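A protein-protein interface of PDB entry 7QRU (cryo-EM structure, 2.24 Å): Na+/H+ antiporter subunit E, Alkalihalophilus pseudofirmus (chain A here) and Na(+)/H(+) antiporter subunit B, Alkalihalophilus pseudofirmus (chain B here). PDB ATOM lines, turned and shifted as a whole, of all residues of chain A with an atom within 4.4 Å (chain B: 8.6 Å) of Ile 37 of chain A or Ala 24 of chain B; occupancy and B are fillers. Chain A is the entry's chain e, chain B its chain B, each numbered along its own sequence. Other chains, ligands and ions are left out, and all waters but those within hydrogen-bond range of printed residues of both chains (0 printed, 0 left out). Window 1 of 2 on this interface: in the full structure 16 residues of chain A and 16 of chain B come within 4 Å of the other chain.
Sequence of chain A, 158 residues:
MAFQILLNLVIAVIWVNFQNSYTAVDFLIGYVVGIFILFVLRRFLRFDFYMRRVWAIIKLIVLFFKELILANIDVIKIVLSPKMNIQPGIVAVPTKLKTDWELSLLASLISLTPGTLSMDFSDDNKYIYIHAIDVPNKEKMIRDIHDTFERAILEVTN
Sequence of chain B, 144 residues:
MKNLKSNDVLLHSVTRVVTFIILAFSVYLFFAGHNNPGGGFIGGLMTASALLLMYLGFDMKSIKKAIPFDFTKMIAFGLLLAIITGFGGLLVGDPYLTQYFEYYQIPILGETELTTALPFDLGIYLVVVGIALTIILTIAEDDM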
ATOM      1  N   ILE A  11     -21.461  -0.678   2.163  1.00  0.00           N
ATOM      2  CA  ILE A  11     -21.452   0.656   1.636  1.00  0.00           C
ATOM      3  C   ILE A  11     -20.333   1.457   2.289  1.00  0.00           C
ATOM      4  O   ILE A  11     -19.644   2.285   1.641  1.00  0.00           O
ATOM      5  CB  ILE A  11     -22.779   1.420   1.743  1.00  0.00           C
ATOM      6  CG1 ILE A  11     -23.905   0.861   0.889  1.00  0.00           C
ATOM      7  CG2 ILE A  11     -22.542   2.932   1.463  1.00  0.00           C
ATOM      8  CD1 ILE A  11     -23.566   0.856  -0.551  1.00  0.00           C
ATOM      9  N   VAL A  33     -24.540   7.556   4.983  1.00  0.00           N
ATOM     10  CA  VAL A  33     -24.782   7.469   3.552  1.00  0.00           C
ATOM     11  C   VAL A  33     -25.438   6.144   3.197  1.00  0.00           C
ATOM     12  O   VAL A  33     -26.446   6.064   2.522  1.00  0.00           O
ATOM     13  CB  VAL A  33     -23.534   7.647   2.718  1.00  0.00           C
ATOM     14  CG1 VAL A  33     -23.829   7.212   1.303  1.00  0.00           C
ATOM     15  CG2 VAL A  33     -23.090   9.113   2.760  1.00  0.00           C
ATOM     16  N   GLY A  34     -24.963   5.071   3.702  1.00  0.00           N
ATOM     17  CA  GLY A  34     -25.611   3.823   3.350  1.00  0.00           C
ATOM     18  C   GLY A  34     -27.003   3.729   3.902  1.00  0.00           C
ATOM     19  O   GLY A  34     -27.808   3.100   3.246  1.00  0.00           O
ATOM     20  N   ILE A  35     -27.299   4.343   5.088  1.00  0.00           N
ATOM     21  CA  ILE A  35     -28.672   4.305   5.645  1.00  0.00           C
ATOM     22  C   ILE A  35     -29.625   5.008   4.690  1.00  0.00           C
ATOM     23  O   ILE A  35     -30.645   4.471   4.356  1.00  0.00           O
ATOM     24  CB  ILE A  35     -28.734   4.974   7.046  1.00  0.00           C
ATOM     25  CG1 ILE A  35     -27.891   4.190   8.046  1.00  0.00           C
ATOM     26  CG2 ILE A  35     -30.063   5.161   7.604  1.00  0.00           C
ATOM     27  CD1 ILE A  35     -27.798   4.962   9.321  1.00  0.00           C
ATOM     28  N   PHE A  36     -29.177   6.156   4.176  1.00  0.00           N
ATOM     29  CA  PHE A  36     -29.974   6.946   3.278  1.00  0.00           C
ATOM     30  C   PHE A  36     -30.221   6.169   1.976  1.00  0.00           C
ATOM     31  O   PHE A  36     -31.358   6.154   1.506  1.00  0.00           O
ATOM     32  CB  PHE A  36     -29.288   8.286   3.054  1.00  0.00           C
ATOM     33  CG  PHE A  36     -29.731   9.025   1.813  1.00  0.00           C
ATOM     34  CD1 PHE A  36     -30.949   9.725   1.805  1.00  0.00           C
ATOM     35  CD2 PHE A  36     -28.933   9.045   0.666  1.00  0.00           C
ATOM     36  CE1 PHE A  36     -31.361  10.409   0.669  1.00  0.00           C
ATOM     37  CE2 PHE A  36     -29.366   9.697  -0.482  1.00  0.00           C
ATOM     38  CZ  PHE A  36     -30.569  10.377  -0.476  1.00  0.00           C
ATOM     39  N   ILE A  37     -29.186   5.511   1.420  1.00  0.00           N
ATOM     40  CA  ILE A  37     -29.314   4.703   0.204  1.00  0.00           C
ATOM     41  C   ILE A  37     -30.298   3.570   0.402  1.00  0.00           C
ATOM     42  O   ILE A  37     -31.186   3.384  -0.419  1.00  0.00           O
ATOM     43  CB  ILE A  37     -27.931   4.226  -0.257  1.00  0.00           C
ATOM     44  CG1 ILE A  37     -27.084   5.443  -0.670  1.00  0.00           C
ATOM     45  CG2 ILE A  37     -27.977   3.207  -1.381  1.00  0.00           C
ATOM     46  CD1 ILE A  37     -25.688   5.047  -0.845  1.00  0.00           C
ATOM     47  N   LEU A  38     -30.214   2.923   1.560  1.00  0.00           N
ATOM     48  CA  LEU A  38     -31.074   1.787   1.833  1.00  0.00           C
ATOM     49  C   LEU A  38     -32.517   2.230   1.996  1.00  0.00           C
ATOM     50  O   LEU A  38     -33.446   1.600   1.533  1.00  0.00           O
ATOM     51  CB  LEU A  38     -30.557   1.103   3.094  1.00  0.00           C
ATOM     52  CG  LEU A  38     -29.351   0.171   2.897  1.00  0.00           C
ATOM     53  CD1 LEU A  38     -28.760  -0.313   4.211  1.00  0.00           C
ATOM     54  CD2 LEU A  38     -29.780  -1.003   2.162  1.00  0.00           C
ATOM     55  N   PHE A  39     -32.697   3.417   2.564  1.00  0.00           N
ATOM     56  CA  PHE A  39     -34.024   3.988   2.722  1.00  0.00           C
ATOM     57  C   PHE A  39     -34.622   4.318   1.349  1.00  0.00           C
ATOM     58  O   PHE A  39     -35.808   4.153   1.101  1.00  0.00           O
ATOM     59  CB  PHE A  39     -33.932   5.247   3.600  1.00  0.00           C
ATOM     60  CG  PHE A  39     -35.243   5.897   3.912  1.00  0.00           C
ATOM     61  CD1 PHE A  39     -36.126   5.267   4.748  1.00  0.00           C
ATOM     62  CD2 PHE A  39     -35.636   7.032   3.236  1.00  0.00           C
ATOM     63  CE1 PHE A  39     -37.319   5.882   5.038  1.00  0.00           C
ATOM     64  CE2 PHE A  39     -36.879   7.556   3.434  1.00  0.00           C
ATOM     65  CZ  PHE A  39     -37.647   7.042   4.419  1.00  0.00           C
ATOM     66  N   VAL A  40     -33.832   4.944   0.479  1.00  0.00           N
ATOM     67  CA  VAL A  40     -34.321   5.310  -0.848  1.00  0.00           C
ATOM     68  C   VAL A  40     -34.719   4.037  -1.620  1.00  0.00           C
ATOM     69  O   VAL A  40     -35.688   4.060  -2.373  1.00  0.00           O
ATOM     70  CB  VAL A  40     -33.284   6.154  -1.592  1.00  0.00           C
ATOM     71  CG1 VAL A  40     -33.623   6.329  -3.023  1.00  0.00           C
ATOM     72  CG2 VAL A  40     -33.251   7.498  -0.949  1.00  0.00           C
ATOM     73  N   LEU A  41     -33.955   2.951  -1.456  1.00  0.00           N
ATOM     74  CA  LEU A  41     -34.195   1.763  -2.233  1.00  0.00           C
ATOM     75  C   LEU A  41     -35.097   0.764  -1.531  1.00  0.00           C
ATOM     76  O   LEU A  41     -35.195  -0.371  -1.993  1.00  0.00           O
ATOM     77  CB  LEU A  41     -32.824   1.168  -2.609  1.00  0.00           C
ATOM     78  CG  LEU A  41     -32.018   2.063  -3.568  1.00  0.00           C
ATOM     79  CD1 LEU A  41     -30.721   1.382  -3.891  1.00  0.00           C
ATOM     80  CD2 LEU A  41     -32.816   2.387  -4.816  1.00  0.00           C
ATOM     81  N   VAL B  17     -27.883  -4.853  -8.309  1.00  0.00           N
ATOM     82  CA  VAL B  17     -26.597  -4.691  -7.636  1.00  0.00           C
ATOM     83  C   VAL B  17     -25.966  -3.360  -8.055  1.00  0.00           C
ATOM     84  O   VAL B  17     -25.526  -2.586  -7.266  1.00  0.00           O
ATOM     85  CB  VAL B  17     -25.683  -5.882  -7.980  1.00  0.00           C
ATOM     86  CG1 VAL B  17     -24.253  -5.691  -7.516  1.00  0.00           C
ATOM     87  CG2 VAL B  17     -26.281  -7.168  -7.454  1.00  0.00           C
ATOM     88  N   VAL B  18     -25.899  -3.093  -9.343  1.00  0.00           N
ATOM     89  CA  VAL B  18     -25.256  -1.914  -9.828  1.00  0.00           C
ATOM     90  C   VAL B  18     -25.931  -0.630  -9.311  1.00  0.00           C
ATOM     91  O   VAL B  18     -25.219   0.322  -9.079  1.00  0.00           O
ATOM     92  CB  VAL B  18     -25.171  -1.912 -11.365  1.00  0.00           C
ATOM     93  CG1 VAL B  18     -24.315  -3.108 -11.690  1.00  0.00           C
ATOM     94  CG2 VAL B  18     -26.518  -1.969 -11.969  1.00  0.00           C
ATOM     95  N   THR B  19     -27.238  -0.594  -9.128  1.00  0.00           N
ATOM     96  CA  THR B  19     -27.979   0.585  -8.677  1.00  0.00           C
ATOM     97  C   THR B  19     -27.524   1.012  -7.285  1.00  0.00           C
ATOM     98  O   THR B  19     -27.124   2.164  -7.099  1.00  0.00           O
ATOM     99  CB  THR B  19     -29.491   0.317  -8.719  1.00  0.00           C
ATOM    100  OG1 THR B  19     -29.810   0.298 -10.117  1.00  0.00           O
ATOM    101  CG2 THR B  19     -30.319   1.336  -7.978  1.00  0.00           C
ATOM    102  N   PHE B  20     -27.414   0.042  -6.394  1.00  0.00           N
ATOM    103  CA  PHE B  20     -26.817   0.293  -5.115  1.00  0.00           C
ATOM    104  C   PHE B  20     -25.459   1.027  -5.263  1.00  0.00           C
ATOM    105  O   PHE B  20     -25.103   1.926  -4.485  1.00  0.00           O
ATOM    106  CB  PHE B  20     -26.670  -1.025  -4.309  1.00  0.00           C
ATOM    107  CG  PHE B  20     -26.834  -0.875  -2.821  1.00  0.00           C
ATOM    108  CD1 PHE B  20     -28.122  -0.775  -2.348  1.00  0.00           C
ATOM    109  CD2 PHE B  20     -25.787  -0.966  -1.897  1.00  0.00           C
ATOM    110  CE1 PHE B  20     -28.365  -0.609  -0.997  1.00  0.00           C
ATOM    111  CE2 PHE B  20     -26.030  -0.771  -0.547  1.00  0.00           C
ATOM    112  CZ  PHE B  20     -27.318  -0.599  -0.097  1.00  0.00           C
ATOM    113  N   ILE B  21     -24.605   0.528  -6.152  1.00  0.00           N
ATOM    114  CA  ILE B  21     -23.252   1.024  -6.304  1.00  0.00           C
ATOM    115  C   ILE B  21     -23.263   2.385  -6.968  1.00  0.00           C
ATOM    116  O   ILE B  21     -22.519   3.267  -6.490  1.00  0.00           O
ATOM    117  CB  ILE B  21     -22.377   0.017  -7.067  1.00  0.00           C
ATOM    118  CG1 ILE B  21     -22.276  -1.331  -6.344  1.00  0.00           C
ATOM    119  CG2 ILE B  21     -20.979   0.551  -7.236  1.00  0.00           C
ATOM    120  CD1 ILE B  21     -21.828  -2.515  -7.277  1.00  0.00           C
ATOM    121  N   ILE B  22     -24.032   2.552  -8.047  1.00  0.00           N
ATOM    122  CA  ILE B  22     -24.107   3.865  -8.642  1.00  0.00           C
ATOM    123  C   ILE B  22     -24.646   4.892  -7.656  1.00  0.00           C
ATOM    124  O   ILE B  22     -24.105   5.987  -7.595  1.00  0.00           O
ATOM    125  CB  ILE B  22     -24.876   3.868  -9.949  1.00  0.00           C
ATOM    126  CG1 ILE B  22     -24.291   2.798 -10.882  1.00  0.00           C
ATOM    127  CG2 ILE B  22     -24.738   5.222 -10.628  1.00  0.00           C
ATOM    128  CD1 ILE B  22     -25.235   2.446 -12.031  1.00  0.00           C
ATOM    129  N   LEU B  23     -25.717   4.632  -6.931  1.00  0.00           N
ATOM    130  CA  LEU B  23     -26.167   5.638  -6.001  1.00  0.00           C
ATOM    131  C   LEU B  23     -25.098   5.990  -4.960  1.00  0.00           C
ATOM    132  O   LEU B  23     -24.858   7.171  -4.652  1.00  0.00           O
ATOM    133  CB  LEU B  23     -27.369   5.116  -5.295  1.00  0.00           C
ATOM    134  CG  LEU B  23     -28.710   5.399  -5.904  1.00  0.00           C
ATOM    135  CD1 LEU B  23     -29.791   4.865  -4.957  1.00  0.00           C
ATOM    136  CD2 LEU B  23     -28.895   6.873  -6.087  1.00  0.00           C
ATOM    137  N   ALA B  24     -24.443   4.988  -4.393  1.00  0.00           N
ATOM    138  CA  ALA B  24     -23.423   5.307  -3.436  1.00  0.00           C
ATOM    139  C   ALA B  24     -22.361   6.169  -4.108  1.00  0.00           C
ATOM    140  O   ALA B  24     -21.815   7.087  -3.518  1.00  0.00           O
ATOM    141  CB  ALA B  24     -22.844   4.047  -2.853  1.00  0.00           C
ATOM    142  N   PHE B  25     -21.936   5.830  -5.322  1.00  0.00           N
ATOM    143  CA  PHE B  25     -20.944   6.623  -6.009  1.00  0.00           C
ATOM    144  C   PHE B  25     -21.495   8.005  -6.322  1.00  0.00           C
ATOM    145  O   PHE B  25     -20.780   8.987  -6.267  1.00  0.00           O
ATOM    146  CB  PHE B  25     -20.535   5.832  -7.246  1.00  0.00           C
ATOM    147  CG  PHE B  25     -19.451   6.473  -8.034  1.00  0.00           C
ATOM    148  CD1 PHE B  25     -18.281   6.843  -7.420  1.00  0.00           C
ATOM    149  CD2 PHE B  25     -19.593   6.618  -9.406  1.00  0.00           C
ATOM    150  CE1 PHE B  25     -17.288   7.452  -8.173  1.00  0.00           C
ATOM    151  CE2 PHE B  25     -18.534   7.125 -10.157  1.00  0.00           C
ATOM    152  CZ  PHE B  25     -17.424   7.635  -9.525  1.00  0.00           C
ATOM    153  N   SER B  26     -22.756   8.143  -6.674  1.00  0.00           N
ATOM    154  CA  SER B  26     -23.249   9.509  -6.881  1.00  0.00           C
ATOM    155  C   SER B  26     -23.205  10.355  -5.628  1.00  0.00           C
ATOM    156  O   SER B  26     -22.985  11.536  -5.749  1.00  0.00           O
ATOM    157  CB  SER B  26     -24.589   9.474  -7.432  1.00  0.00           C
ATOM    158  OG  SER B  26     -25.497   9.105  -6.447  1.00  0.00           O
ATOM    159  N   VAL B  27     -23.493   9.803  -4.463  1.00  0.00           N
ATOM    160  CA  VAL B  27     -23.381  10.603  -3.259  1.00  0.00           C
ATOM    161  C   VAL B  27     -21.923  10.937  -2.987  1.00  0.00           C
ATOM    162  O   VAL B  27     -21.652  12.014  -2.538  1.00  0.00           O
ATOM    163  CB  VAL B  27     -24.037   9.908  -2.054  1.00  0.00           C
ATOM    164  CG1 VAL B  27     -23.787  10.657  -0.780  1.00  0.00           C
ATOM    165  CG2 VAL B  27     -25.476   9.671  -2.346  1.00  0.00           C
ATOM    166  N   TYR B  28     -20.993  10.018  -3.170  1.00  0.00           N
ATOM    167  CA  TYR B  28     -19.597  10.373  -2.995  1.00  0.00           C
ATOM    168  C   TYR B  28     -19.221  11.522  -3.941  1.00  0.00           C
ATOM    169  O   TYR B  28     -18.459  12.373  -3.527  1.00  0.00           O
ATOM    170  CB  TYR B  28     -18.767   9.098  -3.258  1.00  0.00           C
ATOM    171  CG  TYR B  28     -17.327   9.369  -3.528  1.00  0.00           C
ATOM    172  CD1 TYR B  28     -16.488   9.672  -2.488  1.00  0.00           C
ATOM    173  CD2 TYR B  28     -16.870   9.459  -4.843  1.00  0.00           C
ATOM    174  CE1 TYR B  28     -15.198  10.098  -2.744  1.00  0.00           C
ATOM    175  CE2 TYR B  28     -15.584   9.908  -5.117  1.00  0.00           C
ATOM    176  CZ  TYR B  28     -14.764  10.246  -4.056  1.00  0.00           C
ATOM    177  OH  TYR B  28     -13.493  10.707  -4.298  1.00  0.00           O
ATOM    178  N   LEU B  29     -19.556  11.465  -5.234  1.00  0.00           N
ATOM    179  CA  LEU B  29     -19.243  12.507  -6.188  1.00  0.00           C
ATOM    180  C   LEU B  29     -19.803  13.835  -5.719  1.00  0.00           C
ATOM    181  O   LEU B  29     -19.032  14.762  -5.602  1.00  0.00           O
ATOM    182  CB  LEU B  29     -19.814  12.123  -7.548  1.00  0.00           C
ATOM    183  CG  LEU B  29     -18.987  11.022  -8.240  1.00  0.00           C
ATOM    184  CD1 LEU B  29     -19.734  10.496  -9.439  1.00  0.00           C
ATOM    185  CD2 LEU B  29     -17.627  11.537  -8.578  1.00  0.00           C
ATOM    186  N   PHE B  30     -21.045  13.851  -5.205  1.00  0.00           N
ATOM    187  CA  PHE B  30     -21.566  15.085  -4.681  1.00  0.00           C
ATOM    188  C   PHE B  30     -20.687  15.595  -3.543  1.00  0.00           C
ATOM    189  O   PHE B  30     -20.305  16.733  -3.564  1.00  0.00           O
ATOM    190  CB  PHE B  30     -22.995  14.871  -4.219  1.00  0.00           C
ATOM    191  CG  PHE B  30     -23.529  16.036  -3.437  1.00  0.00           C
ATOM    192  CD1 PHE B  30     -23.851  17.249  -4.058  1.00  0.00           C
ATOM    193  CD2 PHE B  30     -23.540  15.993  -2.054  1.00  0.00           C
ATOM    194  CE1 PHE B  30     -24.301  18.315  -3.300  1.00  0.00           C
ATOM    195  CE2 PHE B  30     -23.951  17.082  -1.295  1.00  0.00           C
ATOM    196  CZ  PHE B  30     -24.396  18.218  -1.912  1.00  0.00           C
ATOM    197  N   PHE B  31     -20.390  14.810  -2.494  1.00  0.00           N
ATOM    198  CA  PHE B  31     -19.659  15.384  -1.379  1.00  0.00           C
ATOM    199  C   PHE B  31     -18.201  15.661  -1.720  1.00  0.00           C
ATOM    200  O   PHE B  31     -17.525  16.213  -0.928  1.00  0.00           O
ATOM    201  CB  PHE B  31     -19.692  14.445  -0.181  1.00  0.00           C
ATOM    202  CG  PHE B  31     -20.986  14.544   0.545  1.00  0.00           C
ATOM    203  CD1 PHE B  31     -21.264  15.664   1.296  1.00  0.00           C
ATOM    204  CD2 PHE B  31     -21.981  13.608   0.348  1.00  0.00           C
ATOM    205  CE1 PHE B  31     -22.484  15.773   1.942  1.00  0.00           C
ATOM    206  CE2 PHE B  31     -23.206  13.718   0.981  1.00  0.00           C
ATOM    207  CZ  PHE B  31     -23.452  14.806   1.772  1.00  0.00           C
ATOM    208  N   GLY B  43     -22.663  14.818  -9.478  1.00  0.00           N
ATOM    209  CA  GLY B  43     -23.380  13.971  -8.557  1.00  0.00           C
ATOM    210  C   GLY B  43     -24.790  13.779  -9.036  1.00  0.00           C
ATOM    211  O   GLY B  43     -25.268  12.676  -9.035  1.00  0.00           O
ATOM    212  N   MET B  46     -25.015  11.662 -12.097  1.00  0.00           N
ATOM    213  CA  MET B  46     -24.762  10.290 -11.709  1.00  0.00           C
ATOM    214  C   MET B  46     -25.926   9.643 -11.001  1.00  0.00           C
ATOM    215  O   MET B  46     -26.301   8.499 -11.299  1.00  0.00           O
ATOM    216  CB  MET B  46     -23.506  10.189 -10.887  1.00  0.00           C
ATOM    217  CG  MET B  46     -23.010   8.746 -10.623  1.00  0.00           C
ATOM    218  SD  MET B  46     -22.743   7.796 -12.112  1.00  0.00           S
ATOM    219  CE  MET B  46     -21.339   8.619 -12.774  1.00  0.00           C
ATOM    220  N   THR B  47     -26.595  10.394 -10.105  1.00  0.00           N
ATOM    221  CA  THR B  47     -27.787   9.876  -9.442  1.00  0.00           C
ATOM    222  C   THR B  47     -28.931   9.659 -10.403  1.00  0.00           C
ATOM    223  O   THR B  47     -29.557   8.619 -10.425  1.00  0.00           O
ATOM    224  CB  THR B  47     -28.298  10.847  -8.373  1.00  0.00           C
ATOM    225  OG1 THR B  47     -27.270  11.083  -7.397  1.00  0.00           O
ATOM    226  CG2 THR B  47     -29.586  10.372  -7.734  1.00  0.00           C
ATOM    227  N   ALA B  50     -28.386   6.449 -12.159  1.00  0.00           N
ATOM    228  CA  ALA B  50     -28.882   5.309 -11.394  1.00  0.00           C
ATOM    229  C   ALA B  50     -30.408   5.152 -11.492  1.00  0.00           C
ATOM    230  O   ALA B  50     -30.928   4.054 -11.565  1.00  0.00           O
ATOM    231  CB  ALA B  50     -28.438   5.385  -9.976  1.00  0.00           C
ATOM    232  N   ILE B  67     -39.918   4.247  -6.388  1.00  0.00           N
ATOM    233  CA  ILE B  67     -39.220   5.499  -6.160  1.00  0.00           C
ATOM    234  C   ILE B  67     -40.166   6.612  -6.599  1.00  0.00           C
ATOM    235  O   ILE B  67     -40.075   7.222  -7.680  1.00  0.00           O
ATOM    236  CB  ILE B  67     -37.852   5.615  -6.867  1.00  0.00           C
ATOM    237  CG1 ILE B  67     -37.981   5.463  -8.380  1.00  0.00           C
ATOM    238  CG2 ILE B  67     -36.833   4.624  -6.319  1.00  0.00           C
ATOM    239  CD1 ILE B  67     -36.755   5.915  -9.180  1.00  0.00           C
ATOM    240  N   PHE B  69     -40.793   9.893  -6.172  1.00  0.00           N
ATOM    241  CA  PHE B  69     -40.401  11.280  -5.986  1.00  0.00           C
ATOM    242  C   PHE B  69     -41.182  12.185  -6.939  1.00  0.00           C
ATOM    243  O   PHE B  69     -41.591  11.764  -8.015  1.00  0.00           O
ATOM    244  CB  PHE B  69     -38.925  11.537  -6.234  1.00  0.00           C
ATOM    245  CG  PHE B  69     -37.991  10.673  -5.439  1.00  0.00           C
ATOM    246  CD1 PHE B  69     -37.961  10.742  -4.066  1.00  0.00           C
ATOM    247  CD2 PHE B  69     -37.163   9.770  -6.084  1.00  0.00           C
ATOM    248  CE1 PHE B  69     -37.105   9.933  -3.345  1.00  0.00           C
ATOM    249  CE2 PHE B  69     -36.320   8.950  -5.365  1.00  0.00           C
ATOM    250  CZ  PHE B  69     -36.288   9.044  -3.994  1.00  0.00           C
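Printed residues of chain A that touch a printed residue of chain B: Ile 11, Val 33, Ile 37, Leu 38, Val 40 and Leu 41. Hydrophobic or aromatic side chains of chain A within 4 Å of the printed part of chain B: Ile 11, Val 33, Ile 37, Leu 38, Val 40 and Leu 41. Of the 21 printed residues of chain B, 5 touch a printed residue of chain A. Hydrophobic or aromatic side chains of chain B that line the printed part of chain A: Phe 20, Leu 23, Ala 24, Val 27 and Phe 69. Among the printed residues, no Asp or Glu carboxylate lies within 4 Å of a Lys or Arg side-chain nitrogen of the other chain.
Phe 20 of chain B touches Ile 11 of chain A (CE2 to CD1, 3.0 Å). Val 27 of chain B touches Val 33 of chain A (CG1 to CG2, 3.9 Å). Phe 20 of chain B touches Ile 37 of chain A (CE1 to CG2, 3.9 Å). CD1 of Ile 37 of chain A touches CA of Ala 24 of chain B, 3.5 Å away. CD2 of Leu 38 of chain A touches CZ of Phe 20 of chain B, at 3.4 Å. Val 40 of chain A touches Phe 69 of chain B. CD1 of Leu 41 of chain A touches CD1 of Phe 20 of chain B (3.7 Å). Leu 41 of chain A touches Leu 23 of chain B (CD1 to CD1, 3.8 Å).
Of chain B, only Phe 20 (3.9 Å) and Ala 24 (3.5 Å) come within 4 Å of Ile 37 of chain A. Printed residues of chain A within 4 Å of Ala 24 of chain B: Ile 37 (3.5 Å). Of the printed residues of chain B, Val 40 of chain A touches Phe 69. Printed residues of chain A within 4 Å of Phe 69 of chain B: Val 40. Of the printed residues of chain A, Phe 20 of chain B touches Ile 11 (3.0 Å), Ile 37 (3.9 Å), Leu 38 (3.4 Å) and Leu 41 (3.7 Å). The nearest residue of chain B that does not touch Ile 37 of chain A is Leu 23 of chain B (4.3 Å). The nearest printed residue of chain A that does not touch Ala 24 of chain B is Ile 11 of chain A (4.0004 Å).
OG of Ser 26 of chain B sits at hydrogen-bond distance from O of Leu 23 of chain B (2.7 Å).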
